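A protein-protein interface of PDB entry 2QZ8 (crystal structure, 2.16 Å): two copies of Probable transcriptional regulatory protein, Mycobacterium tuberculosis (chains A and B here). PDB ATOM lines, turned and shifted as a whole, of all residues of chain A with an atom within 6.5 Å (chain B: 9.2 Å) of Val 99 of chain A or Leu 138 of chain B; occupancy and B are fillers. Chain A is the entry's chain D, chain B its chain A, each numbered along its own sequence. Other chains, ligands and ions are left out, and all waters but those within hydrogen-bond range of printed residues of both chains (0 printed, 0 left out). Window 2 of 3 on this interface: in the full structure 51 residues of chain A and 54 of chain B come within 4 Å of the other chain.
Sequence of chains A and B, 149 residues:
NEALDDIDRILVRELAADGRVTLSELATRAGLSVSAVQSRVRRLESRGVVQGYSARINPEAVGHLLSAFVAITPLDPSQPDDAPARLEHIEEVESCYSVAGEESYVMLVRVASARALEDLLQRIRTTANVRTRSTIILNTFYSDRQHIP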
ATOM      1  N   TYR A  97      11.561  13.396  21.537  1.00  0.00           N
ATOM      2  CA  TYR A  97      12.196  13.244  20.231  1.00  0.00           C
ATOM      3  C   TYR A  97      13.680  13.468  20.411  1.00  0.00           C
ATOM      4  O   TYR A  97      14.062  14.339  21.177  1.00  0.00           O
ATOM      5  CB  TYR A  97      11.696  14.311  19.240  1.00  0.00           C
ATOM      6  CG  TYR A  97      10.185  14.471  19.138  1.00  0.00           C
ATOM      7  CD1 TYR A  97       9.518  15.440  19.876  1.00  0.00           C
ATOM      8  CD2 TYR A  97       9.433  13.669  18.283  1.00  0.00           C
ATOM      9  CE1 TYR A  97       8.133  15.606  19.780  1.00  0.00           C
ATOM     10  CE2 TYR A  97       8.046  13.812  18.193  1.00  0.00           C
ATOM     11  CZ  TYR A  97       7.406  14.783  18.940  1.00  0.00           C
ATOM     12  OH  TYR A  97       6.039  14.929  18.845  1.00  0.00           O
ATOM     13  N   SER A  98      14.513  12.697  19.716  1.00  0.00           N
ATOM     14  CA  SER A  98      15.905  13.062  19.553  1.00  0.00           C
ATOM     15  C   SER A  98      15.943  14.010  18.373  1.00  0.00           C
ATOM     16  O   SER A  98      15.180  13.833  17.423  1.00  0.00           O
ATOM     17  CB  SER A  98      16.764  11.843  19.250  1.00  0.00           C
ATOM     18  OG  SER A  98      16.169  11.023  18.247  1.00  0.00           O
ATOM     19  N   VAL A  99      16.818  15.012  18.435  1.00  0.00           N
ATOM     20  CA  VAL A  99      16.873  16.044  17.407  1.00  0.00           C
ATOM     21  C   VAL A  99      18.323  16.306  17.027  1.00  0.00           C
ATOM     22  O   VAL A  99      19.235  15.947  17.763  1.00  0.00           O
ATOM     23  CB  VAL A  99      16.199  17.375  17.873  1.00  0.00           C
ATOM     24  CG1 VAL A  99      14.703  17.188  18.030  1.00  0.00           C
ATOM     25  CG2 VAL A  99      16.816  17.905  19.191  1.00  0.00           C
ATOM     26  N   ALA A 100      18.530  16.900  15.857  1.00  0.00           N
ATOM     27  CA  ALA A 100      19.849  17.385  15.480  1.00  0.00           C
ATOM     28  C   ALA A 100      19.960  18.807  16.018  1.00  0.00           C
ATOM     29  O   ALA A 100      18.952  19.431  16.317  1.00  0.00           O
ATOM     30  CB  ALA A 100      20.016  17.349  13.977  1.00  0.00           C
ATOM     31  N   GLY A 101      21.170  19.323  16.160  1.00  0.00           N
ATOM     32  CA  GLY A 101      21.335  20.656  16.710  1.00  0.00           C
ATOM     33  C   GLY A 101      22.029  20.670  18.047  1.00  0.00           C
ATOM     34  O   GLY A 101      22.748  19.739  18.396  1.00  0.00           O
ATOM     35  N   GLU A 102      21.820  21.732  18.816  1.00  0.00           N
ATOM     36  CA  GLU A 102      22.573  21.884  20.050  1.00  0.00           C
ATOM     37  C   GLU A 102      22.101  20.928  21.149  1.00  0.00           C
ATOM     38  O   GLU A 102      22.902  20.379  21.899  1.00  0.00           O
ATOM     39  CB  GLU A 102      22.521  23.330  20.536  1.00  0.00           C
ATOM     40  CG  GLU A 102      23.512  23.622  21.641  1.00  0.00           C
ATOM     41  CD  GLU A 102      23.970  25.066  21.631  1.00  0.00           C
ATOM     42  OE1 GLU A 102      23.765  25.758  22.653  1.00  0.00           O
ATOM     43  OE2 GLU A 102      24.521  25.508  20.593  1.00  0.00           O
ATOM     44  N   GLU A 103      20.799  20.736  21.261  1.00  0.00           N
ATOM     45  CA  GLU A 103      20.308  19.841  22.296  1.00  0.00           C
ATOM     46  C   GLU A 103      20.080  18.425  21.744  1.00  0.00           C
ATOM     47  O   GLU A 103      19.998  18.232  20.534  1.00  0.00           O
ATOM     48  CB  GLU A 103      19.075  20.430  22.968  1.00  0.00           C
ATOM     49  CG  GLU A 103      19.409  21.627  23.874  1.00  0.00           C
ATOM     50  CD  GLU A 103      19.313  22.977  23.169  1.00  0.00           C
ATOM     51  OE1 GLU A 103      18.370  23.165  22.372  1.00  0.00           O
ATOM     52  OE2 GLU A 103      20.176  23.859  23.423  1.00  0.00           O
ATOM     53  N   SER A 104      20.022  17.439  22.637  1.00  0.00           N
ATOM     54  CA  SER A 104      19.877  16.043  22.257  1.00  0.00           C
ATOM     55  C   SER A 104      18.422  15.638  22.047  1.00  0.00           C
ATOM     56  O   SER A 104      18.121  14.878  21.128  1.00  0.00           O
ATOM     57  CB  SER A 104      20.519  15.135  23.312  1.00  0.00           C
ATOM     58  OG  SER A 104      21.880  15.483  23.485  1.00  0.00           O
ATOM     59  N   TYR A 105      17.521  16.126  22.899  1.00  0.00           N
ATOM     60  CA  TYR A 105      16.096  15.792  22.759  1.00  0.00           C
ATOM     61  C   TYR A 105      15.219  17.012  22.967  1.00  0.00           C
ATOM     62  O   TYR A 105      15.608  17.969  23.645  1.00  0.00           O
ATOM     63  CB  TYR A 105      15.652  14.712  23.771  1.00  0.00           C
ATOM     64  CG  TYR A 105      16.584  13.519  23.871  1.00  0.00           C
ATOM     65  CD1 TYR A 105      17.605  13.477  24.825  1.00  0.00           C
ATOM     66  CD2 TYR A 105      16.440  12.435  23.016  1.00  0.00           C
ATOM     67  CE1 TYR A 105      18.464  12.379  24.903  1.00  0.00           C
ATOM     68  CE2 TYR A 105      17.279  11.348  23.089  1.00  0.00           C
ATOM     69  CZ  TYR A 105      18.289  11.325  24.026  1.00  0.00           C
ATOM     70  OH  TYR A 105      19.104  10.230  24.083  1.00  0.00           O
ATOM     71  N   VAL A 106      14.020  16.948  22.403  1.00  0.00           N
ATOM     72  CA  VAL A 106      12.971  17.924  22.664  1.00  0.00           C
ATOM     73  C   VAL A 106      11.764  17.171  23.191  1.00  0.00           C
ATOM     74  O   VAL A 106      11.416  16.114  22.667  1.00  0.00           O
ATOM     75  CB  VAL A 106      12.570  18.674  21.376  1.00  0.00           C
ATOM     76  CG1 VAL A 106      11.409  19.598  21.651  1.00  0.00           C
ATOM     77  CG2 VAL A 106      13.763  19.468  20.830  1.00  0.00           C
ATOM     78  N   GLU B  60       5.565   7.954   8.821  1.00  0.00           N
ATOM     79  CA  GLU B  60       6.461   7.248   7.907  1.00  0.00           C
ATOM     80  C   GLU B  60       5.708   6.330   6.955  1.00  0.00           C
ATOM     81  O   GLU B  60       6.131   6.124   5.819  1.00  0.00           O
ATOM     82  CB  GLU B  60       7.500   6.444   8.683  1.00  0.00           C
ATOM     83  CG  GLU B  60       8.588   7.290   9.333  1.00  0.00           C
ATOM     84  CD  GLU B  60       9.695   6.440   9.920  1.00  0.00           C
ATOM     85  OE1 GLU B  60      10.655   7.006  10.478  1.00  0.00           O
ATOM     86  OE2 GLU B  60       9.607   5.198   9.821  1.00  0.00           O
ATOM     87  N   LEU B  65       8.914  10.837   5.681  1.00  0.00           N
ATOM     88  CA  LEU B  65      10.125  10.185   6.231  1.00  0.00           C
ATOM     89  C   LEU B  65      10.960  11.139   7.040  1.00  0.00           C
ATOM     90  O   LEU B  65      11.816  10.751   7.829  1.00  0.00           O
ATOM     91  CB  LEU B  65      10.887   9.435   5.162  1.00  0.00           C
ATOM     92  CG  LEU B  65      10.189   8.411   4.295  1.00  0.00           C
ATOM     93  CD1 LEU B  65      11.066   7.867   3.193  1.00  0.00           C
ATOM     94  CD2 LEU B  65       9.544   7.294   5.060  1.00  0.00           C
ATOM     95  N   LEU B  66      10.678  12.423   6.777  1.00  0.00           N
ATOM     96  CA  LEU B  66      11.419  13.480   7.509  1.00  0.00           C
ATOM     97  C   LEU B  66      10.490  14.406   8.250  1.00  0.00           C
ATOM     98  O   LEU B  66       9.596  15.022   7.667  1.00  0.00           O
ATOM     99  CB  LEU B  66      12.345  14.148   6.533  1.00  0.00           C
ATOM    100  CG  LEU B  66      12.936  15.508   6.737  1.00  0.00           C
ATOM    101  CD1 LEU B  66      13.151  15.924   8.154  1.00  0.00           C
ATOM    102  CD2 LEU B  66      14.069  15.778   5.793  1.00  0.00           C
ATOM    103  N   SER B  67      10.654  14.501   9.561  1.00  0.00           N
ATOM    104  CA  SER B  67       9.869  15.406  10.386  1.00  0.00           C
ATOM    105  C   SER B  67      10.824  16.423  10.961  1.00  0.00           C
ATOM    106  O   SER B  67      12.021  16.169  11.017  1.00  0.00           O
ATOM    107  CB  SER B  67       9.188  14.660  11.534  1.00  0.00           C
ATOM    108  OG  SER B  67       8.153  13.815  11.077  1.00  0.00           O
ATOM    109  N   ALA B  68      10.304  17.567  11.397  1.00  0.00           N
ATOM    110  CA  ALA B  68      11.162  18.612  11.945  1.00  0.00           C
ATOM    111  C   ALA B  68      10.353  19.671  12.682  1.00  0.00           C
ATOM    112  O   ALA B  68       9.187  19.924  12.334  1.00  0.00           O
ATOM    113  CB  ALA B  68      11.973  19.257  10.830  1.00  0.00           C
ATOM    114  N   PHE B  69      10.960  20.291  13.689  1.00  0.00           N
ATOM    115  CA  PHE B  69      10.391  21.508  14.230  1.00  0.00           C
ATOM    116  C   PHE B  69      10.933  22.672  13.423  1.00  0.00           C
ATOM    117  O   PHE B  69      12.093  22.686  13.037  1.00  0.00           O
ATOM    118  CB  PHE B  69      10.687  21.671  15.725  1.00  0.00           C
ATOM    119  CG  PHE B  69       9.985  20.658  16.587  1.00  0.00           C
ATOM    120  CD1 PHE B  69       8.654  20.825  16.922  1.00  0.00           C
ATOM    121  CD2 PHE B  69      10.647  19.524  17.036  1.00  0.00           C
ATOM    122  CE1 PHE B  69       7.991  19.889  17.702  1.00  0.00           C
ATOM    123  CE2 PHE B  69       9.984  18.584  17.818  1.00  0.00           C
ATOM    124  CZ  PHE B  69       8.654  18.776  18.146  1.00  0.00           C
ATOM    125  N   LEU B 108       5.507  21.882  13.917  1.00  0.00           N
ATOM    126  CA  LEU B 108       5.933  20.533  13.578  1.00  0.00           C
ATOM    127  C   LEU B 108       5.460  20.254  12.159  1.00  0.00           C
ATOM    128  O   LEU B 108       4.286  20.432  11.808  1.00  0.00           O
ATOM    129  CB  LEU B 108       5.351  19.501  14.540  1.00  0.00           C
ATOM    130  CG  LEU B 108       5.581  18.015  14.230  1.00  0.00           C
ATOM    131  CD1 LEU B 108       7.030  17.687  14.053  1.00  0.00           C
ATOM    132  CD2 LEU B 108       4.980  17.118  15.334  1.00  0.00           C
ATOM    133  N   ARG B 133      13.972  28.473  10.917  1.00  0.00           N
ATOM    134  CA  ARG B 133      15.052  27.728  11.546  1.00  0.00           C
ATOM    135  C   ARG B 133      14.568  26.347  11.940  1.00  0.00           C
ATOM    136  O   ARG B 133      13.723  26.189  12.821  1.00  0.00           O
ATOM    137  CB  ARG B 133      15.624  28.445  12.774  1.00  0.00           C
ATOM    138  CG  ARG B 133      16.765  27.649  13.426  1.00  0.00           C
ATOM    139  CD  ARG B 133      17.274  28.266  14.742  1.00  0.00           C
ATOM    140  NE  ARG B 133      16.220  28.290  15.747  1.00  0.00           N
ATOM    141  CZ  ARG B 133      16.034  27.354  16.677  1.00  0.00           C
ATOM    142  NH1 ARG B 133      16.849  26.303  16.754  1.00  0.00           N
ATOM    143  NH2 ARG B 133      15.033  27.476  17.541  1.00  0.00           N
ATOM    144  N   SER B 134      15.160  25.350  11.308  1.00  0.00           N
ATOM    145  CA  SER B 134      14.632  24.002  11.301  1.00  0.00           C
ATOM    146  C   SER B 134      15.454  23.099  12.228  1.00  0.00           C
ATOM    147  O   SER B 134      16.670  23.099  12.176  1.00  0.00           O
ATOM    148  CB  SER B 134      14.695  23.495   9.858  1.00  0.00           C
ATOM    149  OG  SER B 134      13.854  22.384   9.638  1.00  0.00           O
ATOM    150  N   THR B 135      14.778  22.352  13.090  1.00  0.00           N
ATOM    151  CA  THR B 135      15.425  21.361  13.937  1.00  0.00           C
ATOM    152  C   THR B 135      14.900  19.984  13.563  1.00  0.00           C
ATOM    153  O   THR B 135      13.755  19.618  13.855  1.00  0.00           O
ATOM    154  CB  THR B 135      15.115  21.585  15.399  1.00  0.00           C
ATOM    155  OG1 THR B 135      15.701  22.830  15.812  1.00  0.00           O
ATOM    156  CG2 THR B 135      15.670  20.411  16.243  1.00  0.00           C
ATOM    157  N   ILE B 136      15.743  19.213  12.907  1.00  0.00           N
ATOM    158  CA  ILE B 136      15.306  17.941  12.381  1.00  0.00           C
ATOM    159  C   ILE B 136      15.185  16.877  13.476  1.00  0.00           C
ATOM    160  O   ILE B 136      16.051  16.746  14.341  1.00  0.00           O
ATOM    161  CB  ILE B 136      16.222  17.534  11.224  1.00  0.00           C
ATOM    162  CG1 ILE B 136      16.030  18.576  10.101  1.00  0.00           C
ATOM    163  CG2 ILE B 136      15.941  16.096  10.782  1.00  0.00           C
ATOM    164  CD1 ILE B 136      16.725  18.279   8.830  1.00  0.00           C
ATOM    165  N   ILE B 137      14.075  16.145  13.447  1.00  0.00           N
ATOM    166  CA  ILE B 137      13.854  15.057  14.372  1.00  0.00           C
ATOM    167  C   ILE B 137      14.606  13.825  13.855  1.00  0.00           C
ATOM    168  O   ILE B 137      14.513  13.495  12.675  1.00  0.00           O
ATOM    169  CB  ILE B 137      12.347  14.759  14.489  1.00  0.00           C
ATOM    170  CG1 ILE B 137      11.637  15.922  15.195  1.00  0.00           C
ATOM    171  CG2 ILE B 137      12.116  13.422  15.203  1.00  0.00           C
ATOM    172  CD1 ILE B 137      10.126  15.898  15.072  1.00  0.00           C
ATOM    173  N   LEU B 138      15.371  13.161  14.718  1.00  0.00           N
ATOM    174  CA  LEU B 138      16.079  11.962  14.292  1.00  0.00           C
ATOM    175  C   LEU B 138      15.241  10.735  14.629  1.00  0.00           C
ATOM    176  O   LEU B 138      15.194   9.763  13.876  1.00  0.00           O
ATOM    177  CB  LEU B 138      17.471  11.879  14.933  1.00  0.00           C
ATOM    178  CG  LEU B 138      18.380  13.061  14.573  1.00  0.00           C
ATOM    179  CD1 LEU B 138      19.693  13.017  15.330  1.00  0.00           C
ATOM    180  CD2 LEU B 138      18.614  13.092  13.068  1.00  0.00           C
ATOM    181  N   ASN B 139      14.576  10.789  15.775  1.00  0.00           N
ATOM    182  CA  ASN B 139      13.752   9.687  16.208  1.00  0.00           C
ATOM    183  C   ASN B 139      12.668  10.174  17.135  1.00  0.00           C
ATOM    184  O   ASN B 139      12.885  11.088  17.933  1.00  0.00           O
ATOM    185  CB  ASN B 139      14.587   8.617  16.916  1.00  0.00           C
ATOM    186  CG  ASN B 139      13.776   7.378  17.234  1.00  0.00           C
ATOM    187  OD1 ASN B 139      13.157   6.790  16.345  1.00  0.00           O
ATOM    188  ND2 ASN B 139      13.757   6.984  18.502  1.00  0.00           N
ATOM    189  N   THR B 140      11.500   9.554  17.022  1.00  0.00           N
ATOM    190  CA  THR B 140      10.396   9.800  17.940  1.00  0.00           C
ATOM    191  C   THR B 140      10.319   8.625  18.916  1.00  0.00           C
ATOM    192  O   THR B 140       9.980   7.524  18.521  1.00  0.00           O
ATOM    193  CB  THR B 140       9.076   9.902  17.174  1.00  0.00           C
ATOM    194  OG1 THR B 140       9.154  10.978  16.219  1.00  0.00           O
ATOM    195  CG2 THR B 140       7.911  10.119  18.138  1.00  0.00           C
ATOM    196  N   PHE B 141      10.658   8.846  20.182  1.00  0.00           N
ATOM    197  CA  PHE B 141      10.653   7.746  21.146  1.00  0.00           C
ATOM    198  C   PHE B 141       9.247   7.438  21.608  1.00  0.00           C
ATOM    199  O   PHE B 141       8.867   6.281  21.764  1.00  0.00           O
ATOM    200  CB  PHE B 141      11.584   8.054  22.313  1.00  0.00           C
ATOM    201  CG  PHE B 141      13.034   8.078  21.915  1.00  0.00           C
ATOM    202  CD1 PHE B 141      13.800   6.936  21.991  1.00  0.00           C
ATOM    203  CD2 PHE B 141      13.611   9.233  21.423  1.00  0.00           C
ATOM    204  CE1 PHE B 141      15.128   6.947  21.601  1.00  0.00           C
ATOM    205  CE2 PHE B 141      14.925   9.253  21.023  1.00  0.00           C
ATOM    206  CZ  PHE B 141      15.696   8.114  21.117  1.00  0.00           C
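The backbone NH of Ala 100 of chain A is in hydrogen-bond range of the backbone carbonyl oxygen of Ile 136 of chain B. N of Leu 138 of chain B is in hydrogen-bond range of O of Ser 98 of chain A (2.8 Å). O of Asn 139 of chain B lies within hydrogen-bond range of N of Ser 98 of chain A (2.9 Å).
The backbone carbonyl oxygen of Ser 67 of chain B sits at hydrogen-bond distance from the backbone NH of Ile 137 of chain B (3.2 Å). The backbone carbonyl oxygen (O) of Phe 69 of chain B lies within hydrogen-bond range of the backbone NH (N) of Thr 135 of chain B. The backbone NH (N) of Val 106 of chain A sits at hydrogen-bond distance from the backbone carbonyl oxygen (O) of Tyr 97 of chain A (2.9 Å). The backbone carbonyl oxygen of Ser 104 of chain A lies within hydrogen-bond range of the backbone NH of Val 99 of chain A.
Among the printed residues, pairs that only touch across the chains: Tyr 97 of chain A with Phe 69 of chain B (3.6 Å), Tyr 97 of chain A with Ile 137 of chain B (3.97 Å), Tyr 97 of chain A with Asn 139 of chain B (3.2 Å), Tyr 97 of chain A with Thr 140 of chain B (3.4 Å), Ser 98 of chain A with Ile 137 of chain B (3.5 Å), Ser 98 of chain A with Phe 141 of chain B (3.5 Å), Val 99 of chain A with Thr 135 of chain B (3.5 Å), Val 99 of chain A with Ile 136 of chain B (3.3 Å), Val 99 of chain A with Leu 138 of chain B (3.8 Å), Ala 100 of chain A with Thr 135 of chain B (3.4 Å) and Tyr 105 of chain A with Phe 141 of chain B (3.8 Å).
Val 99 of chain A touches just these residues of chain B: Thr 135, Ile 136 and Leu 138. Leu 138 of chain B touches just these residues of chain A: Ser 98 (2.8 Å) and Val 99 (3.8 Å). Of the printed residues of chain B, Ser 98 of chain A touches Ile 137, Leu 138, Asn 139 and Phe 141. Ala 100 of chain A touches just these residues of chain B: Thr 135 and Ile 136. Of the printed residues of chain A, Phe 69 of chain B touches Tyr 97 (3.6 Å). Of the printed residues of chain A, Ile 136 of chain B touches Val 99 and Ala 100. Printed residues of chain A within 4 Å of Asn 139 of chain B: Tyr 97 and Ser 98. Printed residues of chain A within 4 Å of Thr 135 of chain B: Val 99 and Ala 100. Printed residues of chain B within 4 Å of Tyr 105 of chain A: Phe 141. Leu 65 of chain B touches none of the printed residues of chain A. The nearest residue of chain B that does not touch Val 99 of chain A is Ile 137 of chain B (4.3 Å). The nearest residue of chain A that does not touch Leu 138 of chain B is Ala 100 of chain A (4.1 Å).
Of the 10 printed residues of chain A, 5 touch a printed residue of chain B. Among the printed residues, 14 pairs touch across the chains. Among the printed residues, no Asp or Glu carboxylate lies within 4 Å of a Lys or Arg side-chain nitrogen of the other chain.
No position is printed for both chains. Of the 14 pairs that touch across the chains among the printed residues, none has its exchanged pair printed and touching as well.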
